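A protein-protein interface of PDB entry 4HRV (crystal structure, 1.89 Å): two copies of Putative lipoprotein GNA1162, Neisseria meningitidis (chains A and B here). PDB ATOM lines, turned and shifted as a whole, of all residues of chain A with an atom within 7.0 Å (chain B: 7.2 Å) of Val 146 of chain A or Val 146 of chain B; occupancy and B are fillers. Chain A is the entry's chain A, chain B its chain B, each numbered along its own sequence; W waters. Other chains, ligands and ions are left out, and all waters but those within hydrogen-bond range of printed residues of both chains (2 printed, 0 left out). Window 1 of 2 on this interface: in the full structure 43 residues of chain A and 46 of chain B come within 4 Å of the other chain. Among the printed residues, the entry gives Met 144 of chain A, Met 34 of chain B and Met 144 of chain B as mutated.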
ATOM      1  N   SER A 127      -8.879  26.264   9.727  1.00  0.00           N
ATOM      2  CA  SER A 127      -8.053  26.776  10.806  1.00  0.00           C
ATOM      3  C   SER A 127      -6.838  25.887  11.027  1.00  0.00           C
ATOM      4  O   SER A 127      -6.825  24.724  10.612  1.00  0.00           O
ATOM      5  CB  SER A 127      -8.864  26.959  12.096  1.00  0.00           C
ATOM      6  OG  SER A 127      -9.261  25.723  12.652  1.00  0.00           O
ATOM      7  N   ALA A 128      -5.815  26.453  11.656  1.00  0.00           N
ATOM      8  CA  ALA A 128      -4.567  25.741  11.875  1.00  0.00           C
ATOM      9  C   ALA A 128      -3.936  26.177  13.187  1.00  0.00           C
ATOM     10  O   ALA A 128      -3.927  27.362  13.525  1.00  0.00           O
ATOM     11  CB  ALA A 128      -3.621  26.000  10.720  1.00  0.00           C
ATOM     12  N   SER A 129      -3.412  25.219  13.938  1.00  0.00           N
ATOM     13  CA  SER A 129      -2.640  25.563  15.116  1.00  0.00           C
ATOM     14  C   SER A 129      -1.343  24.794  15.080  1.00  0.00           C
ATOM     15  O   SER A 129      -1.352  23.570  14.917  1.00  0.00           O
ATOM     16  CB  SER A 129      -3.416  25.250  16.389  1.00  0.00           C
ATOM     17  OG  SER A 129      -2.608  25.502  17.519  1.00  0.00           O
ATOM     18  N   ILE A 130      -0.235  25.518  15.227  1.00  0.00           N
ATOM     19  CA  ILE A 130       1.097  24.953  15.041  1.00  0.00           C
ATOM     20  C   ILE A 130       2.025  25.342  16.185  1.00  0.00           C
ATOM     21  O   ILE A 130       2.036  26.499  16.632  1.00  0.00           O
ATOM     22  CB  ILE A 130       1.696  25.372  13.686  1.00  0.00           C
ATOM     23  CG1 ILE A 130       0.806  24.860  12.554  1.00  0.00           C
ATOM     24  CG2 ILE A 130       3.085  24.803  13.514  1.00  0.00           C
ATOM     25  CD1 ILE A 130       1.217  25.354  11.196  1.00  0.00           C
ATOM     26  N   SER A 139      11.700  26.104  10.560  1.00  0.00           N
ATOM     27  CA  SER A 139      10.578  26.111   9.631  1.00  0.00           C
ATOM     28  C   SER A 139      10.709  25.032   8.556  1.00  0.00           C
ATOM     29  O   SER A 139       9.717  24.644   7.943  1.00  0.00           O
ATOM     30  CB  SER A 139      10.442  27.486   8.980  1.00  0.00           C
ATOM     31  OG  SER A 139      10.215  28.482   9.961  1.00  0.00           O
ATOM     32  N   LEU A 141      11.666  21.765   9.062  1.00  0.00           N
ATOM     33  CA  LEU A 141      10.963  20.627   9.636  1.00  0.00           C
ATOM     34  C   LEU A 141       9.505  20.945   9.940  1.00  0.00           C
ATOM     35  O   LEU A 141       8.636  20.106   9.743  1.00  0.00           O
ATOM     36  CB  LEU A 141      11.692  20.134  10.885  1.00  0.00           C
ATOM     37  CG  LEU A 141      13.128  19.731  10.543  1.00  0.00           C
ATOM     38  CD1 LEU A 141      13.955  19.527  11.805  1.00  0.00           C
ATOM     39  CD2 LEU A 141      13.116  18.475   9.676  1.00  0.00           C
ATOM     40  N   LEU A 142       9.233  22.150  10.424  1.00  0.00           N
ATOM     41  CA  LEU A 142       7.850  22.547  10.662  1.00  0.00           C
ATOM     42  C   LEU A 142       7.060  22.508   9.359  1.00  0.00           C
ATOM     43  O   LEU A 142       5.908  22.075   9.331  1.00  0.00           O
ATOM     44  CB  LEU A 142       7.765  23.943  11.269  1.00  0.00           C
ATOM     45  CG  LEU A 142       6.922  24.011  12.542  1.00  0.00           C
ATOM     46  CD1 LEU A 142       6.340  25.400  12.728  1.00  0.00           C
ATOM     47  CD2 LEU A 142       5.836  22.953  12.532  1.00  0.00           C
ATOM     48  N   GLY A 143       7.697  22.941   8.278  1.00  0.00           N
ATOM     49  CA  GLY A 143       7.059  22.945   6.977  1.00  0.00           C
ATOM     50  C   GLY A 143       6.731  21.543   6.519  1.00  0.00           C
ATOM     51  O   GLY A 143       5.665  21.298   5.954  1.00  0.00           O
ATOM     52  N   MET A 144       7.651  20.617   6.766  1.00  0.00           N
ATOM     53  CA  MET A 144       7.452  19.231   6.366  1.00  0.00           C
ATOM     54  C   MET A 144       6.272  18.632   7.105  1.00  0.00           C
ATOM     55  O   MET A 144       5.480  17.905   6.521  1.00  0.00           O
ATOM     56  CB  MET A 144       8.713  18.399   6.624  1.00  0.00           C
ATOM     57  CG  MET A 144       8.502  16.900   6.551  1.00  0.00           C
ATOM     58  SD  MET A 144       7.754  16.179   8.219  1.00  0.00           S
ATOM     59  CE  MET A 144       9.105  16.831   9.483  1.00  0.00           C
ATOM     60  N   LEU A 145       6.168  18.937   8.396  1.00  0.00           N
ATOM     61  CA  LEU A 145       5.069  18.427   9.212  1.00  0.00           C
ATOM     62  C   LEU A 145       3.708  18.963   8.750  1.00  0.00           C
ATOM     63  O   LEU A 145       2.787  18.172   8.510  1.00  0.00           O
ATOM     64  CB  LEU A 145       5.296  18.706  10.707  1.00  0.00           C
ATOM     65  CG  LEU A 145       4.108  18.285  11.586  1.00  0.00           C
ATOM     66  CD1 LEU A 145       3.897  16.775  11.517  1.00  0.00           C
ATOM     67  CD2 LEU A 145       4.285  18.735  13.026  1.00  0.00           C
ATOM     68  N   VAL A 146       3.565  20.287   8.610  1.00  0.00           N
ATOM     69  CA  VAL A 146       2.269  20.821   8.163  1.00  0.00           C
ATOM     70  C   VAL A 146       1.893  20.331   6.779  1.00  0.00           C
ATOM     71  O   VAL A 146       0.735  20.053   6.514  1.00  0.00           O
ATOM     72  CB  VAL A 146       2.163  22.380   8.203  1.00  0.00           C
ATOM     73  CG1 VAL A 146       2.341  22.893   9.615  1.00  0.00           C
ATOM     74  CG2 VAL A 146       3.165  23.026   7.256  1.00  0.00           C
ATOM     75  N   SER A 147       2.872  20.246   5.893  1.00  0.00           N
ATOM     76  CA  SER A 147       2.644  19.715   4.558  1.00  0.00           C
ATOM     77  C   SER A 147       2.109  18.282   4.591  1.00  0.00           C
ATOM     78  O   SER A 147       1.205  17.915   3.831  1.00  0.00           O
ATOM     79  CB  SER A 147       3.942  19.787   3.755  1.00  0.00           C
ATOM     80  OG  SER A 147       3.862  18.990   2.589  1.00  0.00           O
ATOM     81  N   ALA A 148       2.678  17.470   5.475  1.00  0.00           N
ATOM     82  CA  ALA A 148       2.254  16.090   5.612  1.00  0.00           C
ATOM     83  C   ALA A 148       0.826  16.037   6.119  1.00  0.00           C
ATOM     84  O   ALA A 148       0.030  15.212   5.673  1.00  0.00           O
ATOM     85  CB  ALA A 148       3.195  15.342   6.568  1.00  0.00           C
ATOM     86  N   VAL A 149       0.496  16.919   7.059  1.00  0.00           N
ATOM     87  CA  VAL A 149      -0.861  16.951   7.605  1.00  0.00           C
ATOM     88  C   VAL A 149      -1.876  17.412   6.544  1.00  0.00           C
ATOM     89  O   VAL A 149      -2.975  16.867   6.450  1.00  0.00           O
ATOM     90  CB  VAL A 149      -0.960  17.825   8.879  1.00  0.00           C
ATOM     91  CG1 VAL A 149      -2.413  18.008   9.295  1.00  0.00           C
ATOM     92  CG2 VAL A 149      -0.179  17.189  10.016  1.00  0.00           C
ATOM     93  N   VAL A 150      -1.500  18.408   5.748  1.00  0.00           N
ATOM     94  CA  VAL A 150      -2.374  18.870   4.667  1.00  0.00           C
ATOM     95  C   VAL A 150      -2.537  17.790   3.587  1.00  0.00           C
ATOM     96  O   VAL A 150      -3.629  17.607   3.041  1.00  0.00           O
ATOM     97  CB  VAL A 150      -1.886  20.196   4.046  1.00  0.00           C
ATOM     98  CG1 VAL A 150      -2.768  20.590   2.861  1.00  0.00           C
ATOM     99  CG2 VAL A 150      -1.895  21.305   5.093  1.00  0.00           C
ATOM    100  N   ASN A 151      -1.457  17.071   3.289  1.00  0.00           N
ATOM    101  CA  ASN A 151      -1.531  15.943   2.365  1.00  0.00           C
ATOM    102  C   ASN A 151      -2.544  14.911   2.830  1.00  0.00           C
ATOM    103  O   ASN A 151      -3.333  14.402   2.040  1.00  0.00           O
ATOM    104  CB  ASN A 151      -0.164  15.271   2.204  1.00  0.00           C
ATOM    105  CG  ASN A 151      -0.240  13.987   1.393  1.00  0.00           C
ATOM    106  OD1 ASN A 151      -0.053  13.996   0.178  1.00  0.00           O
ATOM    107  ND2 ASN A 151      -0.529  12.876   2.066  1.00  0.00           N
ATOM    108  N   GLN A 152      -2.514  14.593   4.119  1.00  0.00           N
ATOM    109  CA  GLN A 152      -3.467  13.640   4.677  1.00  0.00           C
ATOM    110  C   GLN A 152      -4.926  14.102   4.525  1.00  0.00           C
ATOM    111  O   GLN A 152      -5.822  13.304   4.227  1.00  0.00           O
ATOM    112  CB  GLN A 152      -3.157  13.372   6.151  1.00  0.00           C
ATOM    113  CG  GLN A 152      -1.850  12.619   6.383  1.00  0.00           C
ATOM    114  CD  GLN A 152      -1.694  11.414   5.469  1.00  0.00           C
ATOM    115  OE1 GLN A 152      -0.915  11.443   4.516  1.00  0.00           O
ATOM    116  NE2 GLN A 152      -2.440  10.353   5.754  1.00  0.00           N
ATOM    117  N   MET B  34       1.299   8.914   4.159  1.00  0.00           N
ATOM    118  CA  MET B  34       1.954  10.023   4.832  1.00  0.00           C
ATOM    119  C   MET B  34       3.483   9.966   4.719  1.00  0.00           C
ATOM    120  O   MET B  34       4.134  10.987   4.470  1.00  0.00           O
ATOM    121  CB  MET B  34       1.521  10.086   6.290  1.00  0.00           C
ATOM    122  CG  MET B  34       2.215  11.167   7.068  1.00  0.00           C
ATOM    123  SD  MET B  34       1.410  11.394   8.821  1.00  0.00           S
ATOM    124  CE  MET B  34       0.775  13.233   8.624  1.00  0.00           C
ATOM    125  N   TRP B 124      14.786  18.350  17.471  1.00  0.00           N
ATOM    126  CA  TRP B 124      13.679  19.219  17.084  1.00  0.00           C
ATOM    127  C   TRP B 124      12.363  18.555  17.449  1.00  0.00           C
ATOM    128  O   TRP B 124      12.276  17.332  17.467  1.00  0.00           O
ATOM    129  CB  TRP B 124      13.712  19.456  15.575  1.00  0.00           C
ATOM    130  CG  TRP B 124      12.498  20.166  15.046  1.00  0.00           C
ATOM    131  CD1 TRP B 124      12.309  21.513  14.985  1.00  0.00           C
ATOM    132  CD2 TRP B 124      11.312  19.568  14.504  1.00  0.00           C
ATOM    133  NE1 TRP B 124      11.080  21.799  14.438  1.00  0.00           N
ATOM    134  CE2 TRP B 124      10.447  20.624  14.129  1.00  0.00           C
ATOM    135  CE3 TRP B 124      10.905  18.250  14.282  1.00  0.00           C
ATOM    136  CZ2 TRP B 124       9.192  20.401  13.558  1.00  0.00           C
ATOM    137  CZ3 TRP B 124       9.649  18.026  13.715  1.00  0.00           C
ATOM    138  CH2 TRP B 124       8.811  19.101  13.358  1.00  0.00           C
ATOM    139  N   SER B 127       4.310  20.206  16.381  1.00  0.00           N
ATOM    140  CA  SER B 127       3.016  19.585  16.179  1.00  0.00           C
ATOM    141  C   SER B 127       2.111  20.516  15.395  1.00  0.00           C
ATOM    142  O   SER B 127       2.345  21.728  15.329  1.00  0.00           O
ATOM    143  CB  SER B 127       2.373  19.179  17.511  1.00  0.00           C
ATOM    144  OG  SER B 127       2.302  20.267  18.409  1.00  0.00           O
ATOM    145  N   ALA B 128       1.092  19.935  14.779  1.00  0.00           N
ATOM    146  CA  ALA B 128       0.196  20.698  13.931  1.00  0.00           C
ATOM    147  C   ALA B 128      -1.179  20.081  14.018  1.00  0.00           C
ATOM    148  O   ALA B 128      -1.328  18.854  14.020  1.00  0.00           O
ATOM    149  CB  ALA B 128       0.695  20.695  12.496  1.00  0.00           C
ATOM    150  N   SER B 129      -2.185  20.938  14.116  1.00  0.00           N
ATOM    151  CA  SER B 129      -3.553  20.481  14.116  1.00  0.00           C
ATOM    152  C   SER B 129      -4.292  21.382  13.149  1.00  0.00           C
ATOM    153  O   SER B 129      -4.271  22.605  13.291  1.00  0.00           O
ATOM    154  CB  SER B 129      -4.144  20.542  15.528  1.00  0.00           C
ATOM    155  OG  SER B 129      -5.536  20.270  15.514  1.00  0.00           O
ATOM    156  N   ILE B 130      -4.906  20.770  12.144  1.00  0.00           N
ATOM    157  CA  ILE B 130      -5.482  21.510  11.039  1.00  0.00           C
ATOM    158  C   ILE B 130      -6.907  21.041  10.818  1.00  0.00           C
ATOM    159  O   ILE B 130      -7.186  19.836  10.848  1.00  0.00           O
ATOM    160  CB  ILE B 130      -4.631  21.323   9.783  1.00  0.00           C
ATOM    161  CG1 ILE B 130      -3.268  21.978   9.998  1.00  0.00           C
ATOM    162  CG2 ILE B 130      -5.305  21.928   8.590  1.00  0.00           C
ATOM    163  CD1 ILE B 130      -2.231  21.592   8.973  1.00  0.00           C
ATOM    164  N   SER B 139      -7.611  22.097  -0.674  1.00  0.00           N
ATOM    165  CA  SER B 139      -6.211  21.962  -0.264  1.00  0.00           C
ATOM    166  C   SER B 139      -5.410  23.234  -0.504  1.00  0.00           C
ATOM    167  O   SER B 139      -4.518  23.568   0.278  1.00  0.00           O
ATOM    168  CB  SER B 139      -5.549  20.789  -0.994  1.00  0.00           C
ATOM    169  OG  SER B 139      -4.136  20.854  -0.871  1.00  0.00           O
ATOM    170  N   GLY B 140      -5.728  23.938  -1.590  1.00  0.00           N
ATOM    171  CA  GLY B 140      -5.041  25.172  -1.929  1.00  0.00           C
ATOM    172  C   GLY B 140      -5.137  26.195  -0.813  1.00  0.00           C
ATOM    173  O   GLY B 140      -4.124  26.717  -0.354  1.00  0.00           O
ATOM    174  N   LEU B 141      -6.363  26.478  -0.376  1.00  0.00           N
ATOM    175  CA  LEU B 141      -6.596  27.431   0.701  1.00  0.00           C
ATOM    176  C   LEU B 141      -6.056  26.953   2.048  1.00  0.00           C
ATOM    177  O   LEU B 141      -5.520  27.747   2.805  1.00  0.00           O
ATOM    178  CB  LEU B 141      -8.095  27.758   0.809  1.00  0.00           C
ATOM    179  CG  LEU B 141      -8.667  28.380  -0.464  1.00  0.00           C
ATOM    180  CD1 LEU B 141     -10.176  28.577  -0.375  1.00  0.00           C
ATOM    181  CD2 LEU B 141      -7.969  29.709  -0.762  1.00  0.00           C
ATOM    182  N   LEU B 142      -6.221  25.669   2.364  1.00  0.00           N
ATOM    183  CA  LEU B 142      -5.670  25.132   3.606  1.00  0.00           C
ATOM    184  C   LEU B 142      -4.158  25.239   3.572  1.00  0.00           C
ATOM    185  O   LEU B 142      -3.523  25.566   4.571  1.00  0.00           O
ATOM    186  CB  LEU B 142      -6.060  23.667   3.802  1.00  0.00           C
ATOM    187  CG  LEU B 142      -6.803  23.285   5.089  1.00  0.00           C
ATOM    188  CD1 LEU B 142      -6.509  21.829   5.446  1.00  0.00           C
ATOM    189  CD2 LEU B 142      -6.450  24.195   6.239  1.00  0.00           C
ATOM    190  N   GLY B 143      -3.593  24.979   2.400  1.00  0.00           N
ATOM    191  CA  GLY B 143      -2.170  25.145   2.182  1.00  0.00           C
ATOM    192  C   GLY B 143      -1.702  26.554   2.475  1.00  0.00           C
ATOM    193  O   GLY B 143      -0.717  26.749   3.202  1.00  0.00           O
ATOM    194  N   MET B 144      -2.412  27.546   1.932  1.00  0.00           N
ATOM    195  CA  MET B 144      -1.996  28.932   2.131  1.00  0.00           C
ATOM    196  C   MET B 144      -2.123  29.335   3.587  1.00  0.00           C
ATOM    197  O   MET B 144      -1.296  30.084   4.088  1.00  0.00           O
ATOM    198  CB  MET B 144      -2.759  29.912   1.228  1.00  0.00           C
ATOM    199  CG  MET B 144      -4.057  30.421   1.785  1.00  0.00           C
ATOM    200  SD  MET B 144      -3.956  31.822   3.164  1.00  0.00           S
ATOM    201  CE  MET B 144      -5.800  31.576   3.817  1.00  0.00           C
ATOM    202  N   LEU B 145      -3.150  28.835   4.271  1.00  0.00           N
ATOM    203  CA  LEU B 145      -3.284  29.106   5.704  1.00  0.00           C
ATOM    204  C   LEU B 145      -2.148  28.514   6.546  1.00  0.00           C
ATOM    205  O   LEU B 145      -1.577  29.212   7.375  1.00  0.00           O
ATOM    206  CB  LEU B 145      -4.641  28.642   6.246  1.00  0.00           C
ATOM    207  CG  LEU B 145      -4.819  28.941   7.737  1.00  0.00           C
ATOM    208  CD1 LEU B 145      -4.645  30.438   8.025  1.00  0.00           C
ATOM    209  CD2 LEU B 145      -6.166  28.451   8.248  1.00  0.00           C
ATOM    210  N   VAL B 146      -1.833  27.229   6.363  1.00  0.00           N
ATOM    211  CA  VAL B 146      -0.772  26.636   7.167  1.00  0.00           C
ATOM    212  C   VAL B 146       0.519  27.334   6.815  1.00  0.00           C
ATOM    213  O   VAL B 146       1.362  27.568   7.668  1.00  0.00           O
ATOM    214  CB  VAL B 146      -0.631  25.084   6.969  1.00  0.00           C
ATOM    215  CG1 VAL B 146      -1.977  24.408   7.051  1.00  0.00           C
ATOM    216  CG2 VAL B 146       0.039  24.753   5.646  1.00  0.00           C
ATOM    217  N   SER B 147       0.637  27.717   5.552  1.00  0.00           N
ATOM    218  CA  SER B 147       1.858  28.349   5.077  1.00  0.00           C
ATOM    219  C   SER B 147       2.054  29.692   5.745  1.00  0.00           C
ATOM    220  O   SER B 147       3.171  30.064   6.121  1.00  0.00           O
ATOM    221  CB  SER B 147       1.824  28.506   3.561  1.00  0.00           C
ATOM    222  OG  SER B 147       3.059  29.018   3.109  1.00  0.00           O
ATOM    223  N   ALA B 148       0.953  30.423   5.891  1.00  0.00           N
ATOM    224  CA  ALA B 148       0.972  31.713   6.555  1.00  0.00           C
ATOM    225  C   ALA B 148       1.327  31.549   8.024  1.00  0.00           C
ATOM    226  O   ALA B 148       2.069  32.348   8.589  1.00  0.00           O
ATOM    227  CB  ALA B 148      -0.383  32.382   6.422  1.00  0.00           C
ATOM    228  N   VAL B 149       0.785  30.516   8.653  1.00  0.00           N
ATOM    229  CA  VAL B 149       1.029  30.341  10.072  1.00  0.00           C
ATOM    230  C   VAL B 149       2.494  29.969  10.321  1.00  0.00           C
ATOM    231  O   VAL B 149       3.105  30.448  11.270  1.00  0.00           O
ATOM    232  CB  VAL B 149       0.069  29.323  10.707  1.00  0.00           C
ATOM    233  CG1 VAL B 149       0.541  28.965  12.111  1.00  0.00           C
ATOM    234  CG2 VAL B 149      -1.353  29.896  10.733  1.00  0.00           C
ATOM    235  N   VAL B 150       3.061  29.145   9.452  1.00  0.00           N
ATOM    236  CA  VAL B 150       4.472  28.777   9.609  1.00  0.00           C
ATOM    237  C   VAL B 150       5.368  29.999   9.390  1.00  0.00           C
ATOM    238  O   VAL B 150       6.391  30.157  10.056  1.00  0.00           O
ATOM    239  CB  VAL B 150       4.875  27.613   8.686  1.00  0.00           C
ATOM    240  CG1 VAL B 150       6.393  27.437   8.675  1.00  0.00           C
ATOM    241  CG2 VAL B 150       4.212  26.332   9.151  1.00  0.00           C
ATOM    242  N   ASN B 151       4.965  30.880   8.479  1.00  0.00           N
ATOM    243  CA  ASN B 151       5.716  32.110   8.255  1.00  0.00           C
ATOM    244  C   ASN B 151       5.745  32.968   9.516  1.00  0.00           C
ATOM    245  O   ASN B 151       6.782  33.528   9.869  1.00  0.00           O
ATOM    246  CB  ASN B 151       5.132  32.906   7.086  1.00  0.00           C
ATOM    247  CG  ASN B 151       5.955  34.138   6.753  1.00  0.00           C
ATOM    248  OD1 ASN B 151       6.864  34.090   5.924  1.00  0.00           O
ATOM    249  ND2 ASN B 151       5.643  35.251   7.405  1.00  0.00           N
ATOM    250  N   GLN B 152       4.607  33.068  10.199  1.00  0.00           N
ATOM    251  CA  GLN B 152       4.558  33.816  11.453  1.00  0.00           C
ATOM    252  C   GLN B 152       5.490  33.222  12.510  1.00  0.00           C
ATOM    253  O   GLN B 152       6.127  33.955  13.262  1.00  0.00           O
ATOM    254  CB  GLN B 152       3.136  33.901  11.999  1.00  0.00           C
ATOM    255  CG  GLN B 152       2.171  34.653  11.088  1.00  0.00           C
ATOM    256  CD  GLN B 152       2.759  35.952  10.570  1.00  0.00           C
ATOM    257  OE1 GLN B 152       3.240  36.018   9.440  1.00  0.00           O
ATOM    258  NE2 GLN B 152       2.719  36.993  11.394  1.00  0.00           N
ATOM    259  N   ILE B 153       5.555  31.897  12.577  1.00  0.00           N
ATOM    260  CA  ILE B 153       6.446  31.249  13.536  1.00  0.00           C
ATOM    261  C   ILE B 153       7.898  31.520  13.148  1.00  0.00           C
ATOM    262  O   ILE B 153       8.738  31.817  14.002  1.00  0.00           O
ATOM    263  CB  ILE B 153       6.188  29.725  13.629  1.00  0.00           C
ATOM    264  CG1 ILE B 153       4.773  29.456  14.136  1.00  0.00           C
ATOM    265  CG2 ILE B 153       7.192  29.065  14.559  1.00  0.00           C
ATOM    266  CD1 ILE B 153       4.357  27.994  14.077  1.00  0.00           C
HETATM  267  O   HOH W   1      -6.814  24.311  14.632  1.00  0.00           O
HETATM  268  O   HOH W   2      -0.464  22.026  17.532  1.00  0.00           O
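The backbone NH of Met 34 of chain B sits close to the side-chain amide oxygen of Gln 152 of chain A. O of Ser 129 of chain B lies within hydrogen-bond range of N of Ser 129 of chain A.
The side-chain amide oxygen of Gln 152 of chain A sits at hydrogen-bond distance from the side-chain amide nitrogen of Asn 151 of chain A (2.9 Å).
Among the printed residues, merely in contact across the chains: Ser 127 of chain A with Ile 130 of chain B (3.5 Å), Ser 127 of chain A with Leu 145 of chain B (3.6 Å), Ala 128 of chain A with Ser 129 of chain B (3.5 Å), Ala 128 of chain A with Leu 145 of chain B (3.97 Å), Ser 129 of chain A with Ala 128 of chain B (3.4 Å), Ile 130 of chain A with Ser 127 of chain B (3.5 Å), Ile 130 of chain A with Val 149 of chain B (3.8 Å), Ile 130 of chain A with Val 150 of chain B (3.8 Å), Ile 130 of chain A with Ile 153 of chain B (3.5 Å), Leu 141 of chain A with Trp 124 of chain B (3.5 Å), Leu 142 of chain A with Trp 124 of chain B (3.6 Å), Leu 142 of chain A with Ile 153 of chain B (3.5 Å), Leu 145 of chain A with Ser 127 of chain B (3.5 Å), Leu 145 of chain A with Ala 128 of chain B (3.8 Å), Val 146 of chain A with Ala 128 of chain B (3.98 Å), Val 146 of chain A with Val 146 of chain B (3.9 Å), Val 146 of chain A with Val 150 of chain B (3.9 Å), Ala 148 of chain A with Met 34 of chain B (3.6 Å), Val 149 of chain A with Ile 130 of chain B (3.6 Å), Val 150 of chain A with Ile 130 of chain B (3.9 Å), Val 150 of chain A with Ser 139 of chain B (3.98 Å) and Val 150 of chain A with Val 146 of chain B (3.7 Å).
Printed residues of chain B within 4 Å of Ser 129 of chain A: Ala 128 and Ser 129. Printed residues of chain B within 4 Å of Ile 130 of chain A: Ser 127, Val 149, Val 150 and Ile 153. Of the printed residues of chain B, Leu 145 of chain A touches Ser 127 and Ala 128. Leu 142 of chain B touches none of the printed residues of chain A. Val 146 of chain B touches two residues of chain A. Asn 151 of chain B touches none of the printed residues of chain A. The nearest printed residue of chain B that does not touch Val 146 of chain A is Ile 130 of chain B (4.1 Å).
Among the printed residues, no Asp or Glu carboxylate lies within 4 Å of a Lys or Arg side-chain nitrogen of the other chain.
Ser 127 of chain A touches Leu 145 of chain B, and with the chains exchanged Leu 145 of chain A touches Ser 127 of chain B. Ala 128 of chain A touches Ser 129 of chain B, and with the chains exchanged Ser 129 of chain A touches Ala 128 of chain B. Ser 129 of chain B touches its own counterpart, Ser 129 of chain A. Val 146 of chain A touches Val 150 of chain B, and with the chains exchanged Val 150 of chain A touches Val 146 of chain B. 17 positions are printed for both chains.
Water W2 lies within hydrogen-bond range of the backbone carbonyl oxygen of Ser 129 of chain A (3.2 Å) and the side-chain hydroxyl of Ser 127 of chain B (3.4 Å). Water W1 lies within hydrogen-bond range of the backbone carbonyl oxygen (O) of Ser 129 of chain B and the side-chain hydroxyl (OG) of Ser 127 of chain A.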
